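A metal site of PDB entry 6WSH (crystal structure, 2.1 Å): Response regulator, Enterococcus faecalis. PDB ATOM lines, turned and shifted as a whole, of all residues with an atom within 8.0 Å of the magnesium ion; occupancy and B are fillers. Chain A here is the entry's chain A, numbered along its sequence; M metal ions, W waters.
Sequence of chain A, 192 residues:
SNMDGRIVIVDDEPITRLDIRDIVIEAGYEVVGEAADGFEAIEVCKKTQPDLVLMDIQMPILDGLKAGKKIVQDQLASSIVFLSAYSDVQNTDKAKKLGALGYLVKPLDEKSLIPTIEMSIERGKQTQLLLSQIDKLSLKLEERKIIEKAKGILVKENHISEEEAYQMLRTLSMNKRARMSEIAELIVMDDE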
ATOM      1  N   VAL A  10       0.522 -11.370 -10.727  1.00  0.00           N
ATOM      2  CA  VAL A  10       0.116 -11.039  -9.362  1.00  0.00           C
ATOM      3  C   VAL A  10      -1.021 -10.017  -9.430  1.00  0.00           C
ATOM      4  O   VAL A  10      -0.807  -8.851  -9.767  1.00  0.00           O
ATOM      5  CB  VAL A  10       1.292 -10.489  -8.548  1.00  0.00           C
ATOM      6  CG1 VAL A  10       0.879 -10.192  -7.115  1.00  0.00           C
ATOM      7  CG2 VAL A  10       2.465 -11.475  -8.590  1.00  0.00           C
ATOM      8  N   ASP A  11      -2.237 -10.472  -9.090  1.00  0.00           N
ATOM      9  CA  ASP A  11      -3.419  -9.611  -9.035  1.00  0.00           C
ATOM     10  C   ASP A  11      -4.451 -10.322  -8.150  1.00  0.00           C
ATOM     11  O   ASP A  11      -4.579 -11.543  -8.207  1.00  0.00           O
ATOM     12  CB  ASP A  11      -3.978  -9.345 -10.442  1.00  0.00           C
ATOM     13  CG  ASP A  11      -4.978  -8.205 -10.477  1.00  0.00           C
ATOM     14  OD1 ASP A  11      -5.857  -8.152  -9.597  1.00  0.00           O
ATOM     15  OD2 ASP A  11      -4.868  -7.347 -11.373  1.00  0.00           O
ATOM     16  N   ASP A  12      -5.159  -9.546  -7.305  1.00  0.00           N
ATOM     17  CA  ASP A  12      -6.172 -10.149  -6.431  1.00  0.00           C
ATOM     18  C   ASP A  12      -7.419 -10.595  -7.193  1.00  0.00           C
ATOM     19  O   ASP A  12      -8.124 -11.505  -6.719  1.00  0.00           O
ATOM     20  CB  ASP A  12      -6.466  -9.210  -5.256  1.00  0.00           C
ATOM     21  CG  ASP A  12      -6.929  -7.827  -5.678  1.00  0.00           C
ATOM     22  OD1 ASP A  12      -7.988  -7.378  -5.162  1.00  0.00           O
ATOM     23  OD2 ASP A  12      -6.245  -7.184  -6.493  1.00  0.00           O
ATOM     24  N   GLU A  13      -7.716  -9.984  -8.331  1.00  0.00           N
ATOM     25  CA  GLU A  13      -8.845 -10.373  -9.182  1.00  0.00           C
ATOM     26  C   GLU A  13      -8.605 -11.596 -10.082  1.00  0.00           C
ATOM     27  O   GLU A  13      -7.834 -11.523 -11.038  1.00  0.00           O
ATOM     28  CB  GLU A  13      -9.221  -9.186 -10.069  1.00  0.00           C
ATOM     29  CG  GLU A  13     -10.052  -8.081  -9.439  1.00  0.00           C
ATOM     30  CD  GLU A  13     -10.483  -7.057 -10.496  1.00  0.00           C
ATOM     31  OE1 GLU A  13     -10.139  -5.872 -10.313  1.00  0.00           O
ATOM     32  OE2 GLU A  13     -11.115  -7.436 -11.511  1.00  0.00           O
ATOM     33  N   THR A  16      -8.951 -10.740 -13.871  1.00  0.00           N
ATOM     34  CA  THR A  16      -7.838  -9.992 -14.444  1.00  0.00           C
ATOM     35  C   THR A  16      -6.588 -10.853 -14.592  1.00  0.00           C
ATOM     36  O   THR A  16      -5.881 -10.770 -15.623  1.00  0.00           O
ATOM     37  CB  THR A  16      -7.535  -8.785 -13.566  1.00  0.00           C
ATOM     38  OG1 THR A  16      -8.733  -7.998 -13.420  1.00  0.00           O
ATOM     39  CG2 THR A  16      -6.432  -7.940 -14.183  1.00  0.00           C
ATOM     40  N   ALA A  36      -2.292 -13.734  -5.410  1.00  0.00           N
ATOM     41  CA  ALA A  36      -3.386 -12.815  -5.123  1.00  0.00           C
ATOM     42  C   ALA A  36      -3.091 -11.863  -3.972  1.00  0.00           C
ATOM     43  O   ALA A  36      -3.991 -11.104  -3.572  1.00  0.00           O
ATOM     44  CB  ALA A  36      -4.669 -13.580  -4.784  1.00  0.00           C
ATOM     45  N   MET A  55       2.546  -7.059 -11.531  1.00  0.00           N
ATOM     46  CA  MET A  55       1.993  -6.889 -10.197  1.00  0.00           C
ATOM     47  C   MET A  55       1.006  -5.728 -10.119  1.00  0.00           C
ATOM     48  O   MET A  55       1.338  -4.599 -10.514  1.00  0.00           O
ATOM     49  CB  MET A  55       3.117  -6.666  -9.188  1.00  0.00           C
ATOM     50  CG  MET A  55       2.666  -6.621  -7.738  1.00  0.00           C
ATOM     51  SD  MET A  55       3.738  -7.527  -6.607  1.00  0.00           S
ATOM     52  CE  MET A  55       5.375  -6.908  -7.011  1.00  0.00           C
ATOM     53  N   ASP A  56      -0.202  -6.005  -9.613  1.00  0.00           N
ATOM     54  CA  ASP A  56      -1.082  -4.949  -9.146  1.00  0.00           C
ATOM     55  C   ASP A  56      -0.496  -4.344  -7.861  1.00  0.00           C
ATOM     56  O   ASP A  56       0.108  -5.038  -7.041  1.00  0.00           O
ATOM     57  CB  ASP A  56      -2.477  -5.494  -8.872  1.00  0.00           C
ATOM     58  CG  ASP A  56      -3.529  -4.407  -8.740  1.00  0.00           C
ATOM     59  OD1 ASP A  56      -3.152  -3.228  -8.589  1.00  0.00           O
ATOM     60  OD2 ASP A  56      -4.736  -4.722  -8.839  1.00  0.00           O
ATOM     61  N   ILE A  57      -0.692  -3.025  -7.704  1.00  0.00           N
ATOM     62  CA  ILE A  57      -0.342  -2.362  -6.453  1.00  0.00           C
ATOM     63  C   ILE A  57      -1.414  -2.612  -5.392  1.00  0.00           C
ATOM     64  O   ILE A  57      -1.110  -3.026  -4.257  1.00  0.00           O
ATOM     65  CB  ILE A  57      -0.117  -0.857  -6.708  1.00  0.00           C
ATOM     66  CG1 ILE A  57       1.129  -0.691  -7.589  1.00  0.00           C
ATOM     67  CG2 ILE A  57       0.075  -0.113  -5.407  1.00  0.00           C
ATOM     68  CD1 ILE A  57       1.421   0.716  -8.070  1.00  0.00           C
ATOM     69  N   GLN A  58      -2.668  -2.357  -5.732  1.00  0.00           N
ATOM     70  CA  GLN A  58      -3.770  -2.516  -4.777  1.00  0.00           C
ATOM     71  C   GLN A  58      -4.092  -3.993  -4.552  1.00  0.00           C
ATOM     72  O   GLN A  58      -4.682  -4.655  -5.418  1.00  0.00           O
ATOM     73  CB  GLN A  58      -5.003  -1.770  -5.269  1.00  0.00           C
ATOM     74  CG  GLN A  58      -4.943  -0.274  -5.029  1.00  0.00           C
ATOM     75  CD  GLN A  58      -3.871   0.438  -5.804  1.00  0.00           C
ATOM     76  OE1 GLN A  58      -3.595   0.126  -6.966  1.00  0.00           O
ATOM     77  NE2 GLN A  58      -3.217   1.394  -5.165  1.00  0.00           N
ATOM     78  N   MET A  59      -3.670  -4.522  -3.412  1.00  0.00           N
ATOM     79  CA  MET A  59      -3.976  -5.882  -2.973  1.00  0.00           C
ATOM     80  C   MET A  59      -4.226  -5.915  -1.472  1.00  0.00           C
ATOM     81  O   MET A  59      -3.737  -5.058  -0.746  1.00  0.00           O
ATOM     82  CB  MET A  59      -2.826  -6.843  -3.321  1.00  0.00           C
ATOM     83  CG  MET A  59      -2.681  -7.094  -4.811  1.00  0.00           C
ATOM     84  SD  MET A  59      -1.504  -8.402  -5.194  1.00  0.00           S
ATOM     85  CE  MET A  59       0.022  -7.625  -4.642  1.00  0.00           C
ATOM     86  N   PRO A  60      -5.004  -6.886  -1.001  1.00  0.00           N
ATOM     87  CA  PRO A  60      -5.142  -7.066   0.456  1.00  0.00           C
ATOM     88  C   PRO A  60      -3.959  -7.807   1.080  1.00  0.00           C
ATOM     89  O   PRO A  60      -3.108  -8.397   0.408  1.00  0.00           O
ATOM     90  CB  PRO A  60      -6.436  -7.886   0.559  1.00  0.00           C
ATOM     91  CG  PRO A  60      -6.397  -8.759  -0.677  1.00  0.00           C
ATOM     92  CD  PRO A  60      -5.785  -7.878  -1.765  1.00  0.00           C
ATOM     93  N   LEU A  83       0.771  -2.774 -12.498  1.00  0.00           N
ATOM     94  CA  LEU A  83      -0.503  -2.680 -13.209  1.00  0.00           C
ATOM     95  C   LEU A  83      -1.626  -2.206 -12.274  1.00  0.00           C
ATOM     96  O   LEU A  83      -2.305  -3.036 -11.664  1.00  0.00           O
ATOM     97  CB  LEU A  83      -0.838  -4.056 -13.778  1.00  0.00           C
ATOM     98  CG  LEU A  83       0.109  -4.768 -14.732  1.00  0.00           C
ATOM     99  CD1 LEU A  83      -0.459  -6.124 -15.136  1.00  0.00           C
ATOM    100  CD2 LEU A  83       0.378  -3.924 -15.958  1.00  0.00           C
ATOM    101  N   SER A  84      -1.785  -0.889 -12.136  1.00  0.00           N
ATOM    102  CA  SER A  84      -2.719  -0.311 -11.174  1.00  0.00           C
ATOM    103  C   SER A  84      -3.741   0.606 -11.824  1.00  0.00           C
ATOM    104  O   SER A  84      -3.466   1.259 -12.849  1.00  0.00           O
ATOM    105  CB  SER A  84      -1.947   0.469 -10.088  1.00  0.00           C
ATOM    106  OG  SER A  84      -2.812   1.158  -9.193  1.00  0.00           O
ATOM    107  N   ALA A  85      -4.944   0.632 -11.224  1.00  0.00           N
ATOM    108  CA  ALA A  85      -5.911   1.681 -11.538  1.00  0.00           C
ATOM    109  C   ALA A  85      -5.454   3.053 -11.086  1.00  0.00           C
ATOM    110  O   ALA A  85      -6.072   4.049 -11.454  1.00  0.00           O
ATOM    111  CB  ALA A  85      -7.264   1.382 -10.906  1.00  0.00           C
ATOM    112  N   TYR A  86      -4.440   3.136 -10.252  1.00  0.00           N
ATOM    113  CA  TYR A  86      -3.932   4.382  -9.714  1.00  0.00           C
ATOM    114  C   TYR A  86      -2.599   4.751 -10.355  1.00  0.00           C
ATOM    115  O   TYR A  86      -1.760   3.882 -10.619  1.00  0.00           O
ATOM    116  CB  TYR A  86      -3.845   4.244  -8.245  1.00  0.00           C
ATOM    117  CG  TYR A  86      -5.174   4.072  -7.577  1.00  0.00           C
ATOM    118  CD1 TYR A  86      -5.873   5.164  -7.104  1.00  0.00           C
ATOM    119  CD2 TYR A  86      -5.751   2.822  -7.488  1.00  0.00           C
ATOM    120  CE1 TYR A  86      -7.054   4.985  -6.405  1.00  0.00           C
ATOM    121  CE2 TYR A  86      -6.969   2.638  -6.845  1.00  0.00           C
ATOM    122  CZ  TYR A  86      -7.618   3.732  -6.312  1.00  0.00           C
ATOM    123  OH  TYR A  86      -8.838   3.580  -5.688  1.00  0.00           O
ATOM    124  N   LYS A 106      -4.577   0.632 -15.395  1.00  0.00           N
ATOM    125  CA  LYS A 106      -5.819  -0.053 -15.705  1.00  0.00           C
ATOM    126  C   LYS A 106      -6.918   0.937 -16.095  1.00  0.00           C
ATOM    127  O   LYS A 106      -6.913   2.092 -15.663  1.00  0.00           O
ATOM    128  CB  LYS A 106      -6.265  -0.859 -14.494  1.00  0.00           C
ATOM    129  CG  LYS A 106      -5.413  -2.083 -14.201  1.00  0.00           C
ATOM    130  CD  LYS A 106      -5.899  -2.764 -12.924  1.00  0.00           C
ATOM    131  CE  LYS A 106      -5.227  -4.113 -12.701  1.00  0.00           C
ATOM    132  NZ  LYS A 106      -5.712  -4.787 -11.465  1.00  0.00           N
HETATM  133 MG    MG M   1      -6.032  -5.183  -7.009  1.00  0.00          MG
HETATM  134  O   HOH W   1      -7.159  -5.971  -9.035  1.00  0.00           O
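OG of Ser 84 lies within hydrogen-bond range of OE1 of Gln 58 (2.6 Å).
The side-chain carboxylate of Asp 56 lies close to the side-chain amino group of Lys 106 (2.8 Å).
NZ of Lys 106 lies within salt-bridge range of OD2 of Asp 11 (2.7 Å).
The backbone carbonyl oxygen of Val 10 is in hydrogen-bond range of the backbone NH of Asp 56, at 2.9 Å.
OD1 of Asp 11 lies within hydrogen-bond range of N of Glu 13 (2.9 Å).
The magnesium ion is bound by OD2 of Asp 12, 2.1 Å away.
The backbone carbonyl oxygen (O) of Gln 58 binds the magnesium ion, at 2.2 Å.
The magnesium ion is bound by the side-chain carboxylate (OD2) of Asp 56 (2.3 Å).
Water W1 binds the magnesium ion (2.4 Å).
Asp 11 touches the magnesium ion (OD1 to MG, 3.9 Å).
Of the 17 residues printed, 4 come within 4 Å of the magnesium ion.
Water W1 lies within hydrogen-bond range of the side-chain carboxylate (OD1) of Asp 11, the side-chain amino group (NZ) of Lys 106 and the side-chain carboxylate (OE1) of Glu 13.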
